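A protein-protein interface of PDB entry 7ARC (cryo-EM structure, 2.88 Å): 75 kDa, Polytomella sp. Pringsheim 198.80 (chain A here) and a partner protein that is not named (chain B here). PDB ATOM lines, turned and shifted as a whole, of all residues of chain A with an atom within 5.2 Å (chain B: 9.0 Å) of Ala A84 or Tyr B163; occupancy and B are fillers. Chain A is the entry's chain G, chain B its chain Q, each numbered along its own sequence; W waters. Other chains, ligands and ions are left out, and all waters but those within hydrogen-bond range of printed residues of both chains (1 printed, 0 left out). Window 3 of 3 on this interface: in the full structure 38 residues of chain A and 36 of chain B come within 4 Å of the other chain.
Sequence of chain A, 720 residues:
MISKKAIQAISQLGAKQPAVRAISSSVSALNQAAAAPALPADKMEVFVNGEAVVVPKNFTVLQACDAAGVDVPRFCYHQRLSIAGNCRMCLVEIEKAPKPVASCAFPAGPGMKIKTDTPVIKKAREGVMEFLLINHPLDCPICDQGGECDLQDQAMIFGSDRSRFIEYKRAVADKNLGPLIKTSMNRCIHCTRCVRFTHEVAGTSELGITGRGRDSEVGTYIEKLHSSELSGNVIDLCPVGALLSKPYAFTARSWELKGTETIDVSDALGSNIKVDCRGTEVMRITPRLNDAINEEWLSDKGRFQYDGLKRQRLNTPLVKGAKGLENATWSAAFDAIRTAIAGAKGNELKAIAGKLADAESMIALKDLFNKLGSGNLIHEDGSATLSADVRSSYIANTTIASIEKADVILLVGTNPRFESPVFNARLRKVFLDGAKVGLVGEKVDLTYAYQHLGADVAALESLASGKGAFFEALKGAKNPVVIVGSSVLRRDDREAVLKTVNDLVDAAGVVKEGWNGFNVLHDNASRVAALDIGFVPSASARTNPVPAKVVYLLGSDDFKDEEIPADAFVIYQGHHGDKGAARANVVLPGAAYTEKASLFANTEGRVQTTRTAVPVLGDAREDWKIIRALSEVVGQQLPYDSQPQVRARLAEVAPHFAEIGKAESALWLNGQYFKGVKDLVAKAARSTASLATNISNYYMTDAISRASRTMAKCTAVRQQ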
ATOM      1  N   CYS A  76      14.924 -13.428 -29.365  1.00  0.00           N
ATOM      2  CA  CYS A  76      14.295 -13.231 -28.070  1.00  0.00           C
ATOM      3  C   CYS A  76      13.087 -12.319 -28.126  1.00  0.00           C
ATOM      4  O   CYS A  76      12.314 -12.285 -27.164  1.00  0.00           O
ATOM      5  CB  CYS A  76      15.295 -12.637 -27.080  1.00  0.00           C
ATOM      6  SG  CYS A  76      15.867 -10.986 -27.524  1.00  0.00           S
ATOM      7  N   SER A  82       7.120  -9.278 -23.103  1.00  0.00           N
ATOM      8  CA  SER A  82       7.914  -8.105 -22.765  1.00  0.00           C
ATOM      9  C   SER A  82       9.211  -8.091 -23.562  1.00  0.00           C
ATOM     10  O   SER A  82       9.806  -9.137 -23.830  1.00  0.00           O
ATOM     11  CB  SER A  82       8.233  -8.104 -21.273  1.00  0.00           C
ATOM     12  OG  SER A  82       7.058  -7.989 -20.499  1.00  0.00           O
ATOM     13  N   ILE A  83       9.647  -6.894 -23.949  1.00  0.00           N
ATOM     14  CA  ILE A  83      10.907  -6.753 -24.667  1.00  0.00           C
ATOM     15  C   ILE A  83      12.071  -7.105 -23.749  1.00  0.00           C
ATOM     16  O   ILE A  83      12.098  -6.717 -22.574  1.00  0.00           O
ATOM     17  CB  ILE A  83      11.048  -5.331 -25.232  1.00  0.00           C
ATOM     18  CG1 ILE A  83       9.795  -4.947 -26.014  1.00  0.00           C
ATOM     19  CG2 ILE A  83      12.273  -5.228 -26.112  1.00  0.00           C
ATOM     20  CD1 ILE A  83       9.841  -3.560 -26.593  1.00  0.00           C
ATOM     21  N   ALA A  84      13.037  -7.851 -24.281  1.00  0.00           N
ATOM     22  CA  ALA A  84      14.191  -8.301 -23.514  1.00  0.00           C
ATOM     23  C   ALA A  84      15.493  -7.673 -23.989  1.00  0.00           C
ATOM     24  O   ALA A  84      16.212  -7.069 -23.191  1.00  0.00           O
ATOM     25  CB  ALA A  84      14.296  -9.829 -23.575  1.00  0.00           C
ATOM     26  N   GLY A  85      15.819  -7.805 -25.272  1.00  0.00           N
ATOM     27  CA  GLY A  85      17.029  -7.229 -25.820  1.00  0.00           C
ATOM     28  C   GLY A  85      18.306  -7.996 -25.572  1.00  0.00           C
ATOM     29  O   GLY A  85      19.388  -7.437 -25.766  1.00  0.00           O
ATOM     30  N   ASN A  86      18.225  -9.256 -25.150  1.00  0.00           N
ATOM     31  CA  ASN A  86      19.413  -9.995 -24.740  1.00  0.00           C
ATOM     32  C   ASN A  86      20.144 -10.672 -25.898  1.00  0.00           C
ATOM     33  O   ASN A  86      21.375 -10.700 -25.902  1.00  0.00           O
ATOM     34  CB  ASN A  86      19.047 -11.004 -23.647  1.00  0.00           C
ATOM     35  CG  ASN A  86      17.940 -11.932 -24.053  1.00  0.00           C
ATOM     36  OD1 ASN A  86      17.632 -12.065 -25.227  1.00  0.00           O
ATOM     37  ND2 ASN A  86      17.313 -12.562 -23.074  1.00  0.00           N
ATOM     38  N   ALA A 105      14.142  -3.046 -28.939  1.00  0.00           N
ATOM     39  CA  ALA A 105      14.006  -2.159 -27.795  1.00  0.00           C
ATOM     40  C   ALA A 105      14.333  -0.701 -28.085  1.00  0.00           C
ATOM     41  O   ALA A 105      14.234   0.125 -27.173  1.00  0.00           O
ATOM     42  CB  ALA A 105      14.888  -2.657 -26.648  1.00  0.00           C
ATOM     43  N   THR A 192      14.846 -15.204 -23.007  1.00  0.00           N
ATOM     44  CA  THR A 192      14.020 -15.312 -21.814  1.00  0.00           C
ATOM     45  C   THR A 192      12.543 -15.480 -22.152  1.00  0.00           C
ATOM     46  O   THR A 192      11.678 -15.107 -21.360  1.00  0.00           O
ATOM     47  CB  THR A 192      14.257 -14.115 -20.897  1.00  0.00           C
ATOM     48  OG1 THR A 192      13.910 -12.909 -21.581  1.00  0.00           O
ATOM     49  CG2 THR A 192      15.714 -14.054 -20.476  1.00  0.00           C
ATOM     50  N   ARG A 196       9.612 -15.109 -19.493  1.00  0.00           N
ATOM     51  CA  ARG A 196       8.668 -14.013 -19.687  1.00  0.00           C
ATOM     52  C   ARG A 196       7.245 -14.525 -19.856  1.00  0.00           C
ATOM     53  O   ARG A 196       6.299 -13.913 -19.354  1.00  0.00           O
ATOM     54  CB  ARG A 196       9.086 -13.160 -20.881  1.00  0.00           C
ATOM     55  CG  ARG A 196      10.038 -12.044 -20.514  1.00  0.00           C
ATOM     56  CD  ARG A 196      11.112 -11.833 -21.554  1.00  0.00           C
ATOM     57  NE  ARG A 196      10.594 -11.551 -22.884  1.00  0.00           N
ATOM     58  CZ  ARG A 196      11.189 -11.926 -24.008  1.00  0.00           C
ATOM     59  NH1 ARG A 196      12.324 -12.602 -23.996  1.00  0.00           N
ATOM     60  NH2 ARG A 196      10.636 -11.609 -25.172  1.00  0.00           N
ATOM     61  N   ARG B 156       1.948  -4.004 -30.041  1.00  0.00           N
ATOM     62  CA  ARG B 156       2.210  -4.421 -28.672  1.00  0.00           C
ATOM     63  C   ARG B 156       1.159  -3.845 -27.733  1.00  0.00           C
ATOM     64  O   ARG B 156       0.580  -2.786 -27.990  1.00  0.00           O
ATOM     65  CB  ARG B 156       3.603  -3.973 -28.234  1.00  0.00           C
ATOM     66  CG  ARG B 156       4.699  -4.293 -29.233  1.00  0.00           C
ATOM     67  CD  ARG B 156       6.068  -4.259 -28.586  1.00  0.00           C
ATOM     68  NE  ARG B 156       6.019  -4.642 -27.182  1.00  0.00           N
ATOM     69  CZ  ARG B 156       6.193  -5.878 -26.740  1.00  0.00           C
ATOM     70  NH1 ARG B 156       6.422  -6.881 -27.570  1.00  0.00           N
ATOM     71  NH2 ARG B 156       6.130  -6.115 -25.435  1.00  0.00           N
ATOM     72  N   GLN B 157       0.916  -4.553 -26.633  1.00  0.00           N
ATOM     73  CA  GLN B 157      -0.076  -4.113 -25.665  1.00  0.00           C
ATOM     74  C   GLN B 157       0.440  -2.914 -24.872  1.00  0.00           C
ATOM     75  O   GLN B 157       1.640  -2.640 -24.816  1.00  0.00           O
ATOM     76  CB  GLN B 157      -0.456  -5.251 -24.720  1.00  0.00           C
ATOM     77  CG  GLN B 157       0.631  -5.665 -23.755  1.00  0.00           C
ATOM     78  CD  GLN B 157       0.081  -6.445 -22.579  1.00  0.00           C
ATOM     79  OE1 GLN B 157      -0.933  -6.068 -21.992  1.00  0.00           O
ATOM     80  NE2 GLN B 157       0.745  -7.537 -22.230  1.00  0.00           N
ATOM     81  N   ARG B 159       0.595  -2.347 -21.698  1.00  0.00           N
ATOM     82  CA  ARG B 159       1.388  -2.623 -20.504  1.00  0.00           C
ATOM     83  C   ARG B 159       2.871  -2.710 -20.848  1.00  0.00           C
ATOM     84  O   ARG B 159       3.718  -2.188 -20.115  1.00  0.00           O
ATOM     85  CB  ARG B 159       0.893  -3.916 -19.851  1.00  0.00           C
ATOM     86  CG  ARG B 159       1.714  -4.452 -18.680  1.00  0.00           C
ATOM     87  CD  ARG B 159       2.176  -3.364 -17.723  1.00  0.00           C
ATOM     88  NE  ARG B 159       2.987  -3.912 -16.643  1.00  0.00           N
ATOM     89  CZ  ARG B 159       4.164  -3.430 -16.271  1.00  0.00           C
ATOM     90  NH1 ARG B 159       4.692  -2.370 -16.858  1.00  0.00           N
ATOM     91  NH2 ARG B 159       4.826  -4.026 -15.285  1.00  0.00           N
ATOM     92  N   TYR B 160       3.200  -3.341 -21.973  1.00  0.00           N
ATOM     93  CA  TYR B 160       4.583  -3.533 -22.392  1.00  0.00           C
ATOM     94  C   TYR B 160       4.765  -2.964 -23.790  1.00  0.00           C
ATOM     95  O   TYR B 160       5.323  -3.621 -24.672  1.00  0.00           O
ATOM     96  CB  TYR B 160       4.973  -5.010 -22.360  1.00  0.00           C
ATOM     97  CG  TYR B 160       4.806  -5.669 -21.013  1.00  0.00           C
ATOM     98  CD1 TYR B 160       5.616  -5.319 -19.945  1.00  0.00           C
ATOM     99  CD2 TYR B 160       3.848  -6.649 -20.814  1.00  0.00           C
ATOM    100  CE1 TYR B 160       5.472  -5.920 -18.715  1.00  0.00           C
ATOM    101  CE2 TYR B 160       3.695  -7.256 -19.586  1.00  0.00           C
ATOM    102  CZ  TYR B 160       4.510  -6.888 -18.540  1.00  0.00           C
ATOM    103  OH  TYR B 160       4.359  -7.491 -17.315  1.00  0.00           O
ATOM    104  N   LEU B 161       4.286  -1.736 -23.990  1.00  0.00           N
ATOM    105  CA  LEU B 161       4.392  -1.085 -25.290  1.00  0.00           C
ATOM    106  C   LEU B 161       5.840  -0.847 -25.698  1.00  0.00           C
ATOM    107  O   LEU B 161       6.158  -0.863 -26.891  1.00  0.00           O
ATOM    108  CB  LEU B 161       3.618   0.232 -25.259  1.00  0.00           C
ATOM    109  CG  LEU B 161       3.530   1.061 -26.534  1.00  0.00           C
ATOM    110  CD1 LEU B 161       2.803   0.288 -27.613  1.00  0.00           C
ATOM    111  CD2 LEU B 161       2.820   2.365 -26.240  1.00  0.00           C
ATOM    112  N   GLY B 162       6.731  -0.637 -24.732  1.00  0.00           N
ATOM    113  CA  GLY B 162       8.126  -0.403 -25.034  1.00  0.00           C
ATOM    114  C   GLY B 162       9.012  -0.982 -23.954  1.00  0.00           C
ATOM    115  O   GLY B 162       8.539  -1.465 -22.924  1.00  0.00           O
ATOM    116  N   TYR B 163      10.320  -0.940 -24.213  1.00  0.00           N
ATOM    117  CA  TYR B 163      11.275  -1.439 -23.231  1.00  0.00           C
ATOM    118  C   TYR B 163      11.235  -0.633 -21.943  1.00  0.00           C
ATOM    119  O   TYR B 163      11.431  -1.191 -20.858  1.00  0.00           O
ATOM    120  CB  TYR B 163      12.686  -1.435 -23.809  1.00  0.00           C
ATOM    121  CG  TYR B 163      13.686  -2.110 -22.906  1.00  0.00           C
ATOM    122  CD1 TYR B 163      13.741  -3.491 -22.811  1.00  0.00           C
ATOM    123  CD2 TYR B 163      14.559  -1.366 -22.130  1.00  0.00           C
ATOM    124  CE1 TYR B 163      14.645  -4.110 -21.977  1.00  0.00           C
ATOM    125  CE2 TYR B 163      15.463  -1.975 -21.294  1.00  0.00           C
ATOM    126  CZ  TYR B 163      15.504  -3.347 -21.222  1.00  0.00           C
ATOM    127  OH  TYR B 163      16.410  -3.958 -20.388  1.00  0.00           O
ATOM    128  N   GLY B 164      10.995   0.674 -22.037  1.00  0.00           N
ATOM    129  CA  GLY B 164      10.899   1.488 -20.839  1.00  0.00           C
ATOM    130  C   GLY B 164       9.754   1.088 -19.933  1.00  0.00           C
ATOM    131  O   GLY B 164       9.863   1.184 -18.710  1.00  0.00           O
ATOM    132  N   ASP B 165       8.653   0.610 -20.514  1.00  0.00           N
ATOM    133  CA  ASP B 165       7.489   0.208 -19.733  1.00  0.00           C
ATOM    134  C   ASP B 165       7.777  -0.959 -18.799  1.00  0.00           C
ATOM    135  O   ASP B 165       7.021  -1.170 -17.846  1.00  0.00           O
ATOM    136  CB  ASP B 165       6.333  -0.142 -20.666  1.00  0.00           C
ATOM    137  CG  ASP B 165       5.781   1.073 -21.380  1.00  0.00           C
ATOM    138  OD1 ASP B 165       5.860   2.179 -20.811  1.00  0.00           O
ATOM    139  OD2 ASP B 165       5.266   0.924 -22.507  1.00  0.00           O
ATOM    140  N   ASN B 166       8.837  -1.729 -19.052  1.00  0.00           N
ATOM    141  CA  ASN B 166       9.171  -2.834 -18.161  1.00  0.00           C
ATOM    142  C   ASN B 166       9.522  -2.337 -16.766  1.00  0.00           C
ATOM    143  O   ASN B 166       9.169  -2.973 -15.767  1.00  0.00           O
ATOM    144  CB  ASN B 166      10.340  -3.638 -18.730  1.00  0.00           C
ATOM    145  CG  ASN B 166      10.009  -4.298 -20.041  1.00  0.00           C
ATOM    146  OD1 ASN B 166       9.158  -5.180 -20.106  1.00  0.00           O
ATOM    147  ND2 ASN B 166      10.684  -3.875 -21.099  1.00  0.00           N
ATOM    148  N   TYR B 167      10.220  -1.207 -16.678  1.00  0.00           N
ATOM    149  CA  TYR B 167      10.676  -0.655 -15.411  1.00  0.00           C
ATOM    150  C   TYR B 167       9.915   0.610 -15.026  1.00  0.00           C
ATOM    151  O   TYR B 167      10.466   1.497 -14.374  1.00  0.00           O
ATOM    152  CB  TYR B 167      12.174  -0.383 -15.476  1.00  0.00           C
ATOM    153  CG  TYR B 167      12.931  -1.471 -16.197  1.00  0.00           C
ATOM    154  CD1 TYR B 167      13.200  -2.682 -15.580  1.00  0.00           C
ATOM    155  CD2 TYR B 167      13.368  -1.289 -17.501  1.00  0.00           C
ATOM    156  CE1 TYR B 167      13.885  -3.678 -16.238  1.00  0.00           C
ATOM    157  CE2 TYR B 167      14.053  -2.279 -18.165  1.00  0.00           C
ATOM    158  CZ  TYR B 167      14.310  -3.471 -17.529  1.00  0.00           C
ATOM    159  OH  TYR B 167      14.995  -4.463 -18.190  1.00  0.00           O
ATOM    160  N   SER B 168       8.655   0.706 -15.435  1.00  0.00           N
ATOM    161  CA  SER B 168       7.825   1.850 -15.107  1.00  0.00           C
ATOM    162  C   SER B 168       7.276   1.738 -13.689  1.00  0.00           C
ATOM    163  O   SER B 168       7.376   0.700 -13.032  1.00  0.00           O
ATOM    164  CB  SER B 168       6.680   1.976 -16.108  1.00  0.00           C
ATOM    165  OG  SER B 168       5.839   3.068 -15.787  1.00  0.00           O
ATOM    166  N   ARG B 171       4.299  -0.994 -12.339  1.00  0.00           N
ATOM    167  CA  ARG B 171       4.422  -2.312 -11.729  1.00  0.00           C
ATOM    168  C   ARG B 171       3.756  -2.351 -10.359  1.00  0.00           C
ATOM    169  O   ARG B 171       2.971  -3.258 -10.060  1.00  0.00           O
ATOM    170  CB  ARG B 171       5.898  -2.689 -11.615  1.00  0.00           C
ATOM    171  CG  ARG B 171       6.653  -2.626 -12.926  1.00  0.00           C
ATOM    172  CD  ARG B 171       8.150  -2.548 -12.704  1.00  0.00           C
ATOM    173  NE  ARG B 171       8.519  -1.398 -11.888  1.00  0.00           N
ATOM    174  CZ  ARG B 171       9.733  -1.184 -11.400  1.00  0.00           C
ATOM    175  NH1 ARG B 171      10.728  -2.023 -11.630  1.00  0.00           N
ATOM    176  NH2 ARG B 171       9.954  -0.099 -10.667  1.00  0.00           N
HETATM  177  O   HOH W   1       8.380  -3.950 -22.675  1.00  0.00           O
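Water W1 lies within hydrogen-bond range of O of Gly B162, ND2 of Asn B166 and N of Ile A83.
Hydrophobic or aromatic side chains of chain A within 4 Å of the printed part of chain B: Ile A83 and Ala A105.
Of the 13 printed residues of chain B, 5 touch a printed residue of chain A.
Printed residues of chain B that touch a printed residue of chain A: Arg B156, Tyr B160, Gly B162, Tyr B163 and Asn B166.
CA of Ser A82 touches NH2 of Arg B156, 3.8 Å away.
CD1 of Tyr B160 touches OG of Ser A82, 3.1 Å away.
Asn B166 touches Ser A82.
Ile A83 touches Arg B156 (CG1 to CZ, 3.8 Å).
Gly B162 touches Ile A83 (C to CD1, 3.8 Å).
Tyr B163 touches Ile A83 (N to CD1, 3.6 Å).
O of Ile A83 touches ND2 of Asn B166 (3.5 Å).
Ala A84 touches Tyr B163.
CB of Tyr B163 touches CB of Ala A105 (3.8 Å).
Of chain B, only Arg B156 (3.8 Å), Gly B162 (3.8 Å), Tyr B163 (3.6 Å) and Asn B166 (3.5 Å) come within 4 Å of Ile A83.
Ala A84 touches just one residue of chain B: Tyr B163 (3.6 Å).
No residue of chain B comes within 4 Å of Gly A85.
Printed residues of chain A within 4 Å of Arg B156: Ser A82 (3.8 Å) and Ile A83 (3.8 Å).
Of the printed residues of chain A, Tyr B160 touches Ser A82.
Leu B161 touches none of the printed residues of chain A.
The backbone carbonyl oxygen (O) of Ser A82 is in hydrogen-bond range of the guanidinium group (NE) of Arg A196 (2.7 Å).
NH2 of Arg B156 lies within hydrogen-bond range of O of Tyr B160.
The side-chain carboxylate of Asp B165 lies within hydrogen-bond range of the backbone NH of Gly B162, 3.1 Å away.
The backbone carbonyl oxygen (O) of Tyr B163 lies within hydrogen-bond range of the side-chain amide nitrogen (ND2) of Asn B166 (2.8 Å).
The side-chain hydroxyl of Tyr B163 sits at hydrogen-bond distance from the side-chain hydroxyl of Tyr B167 (2.7 Å).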
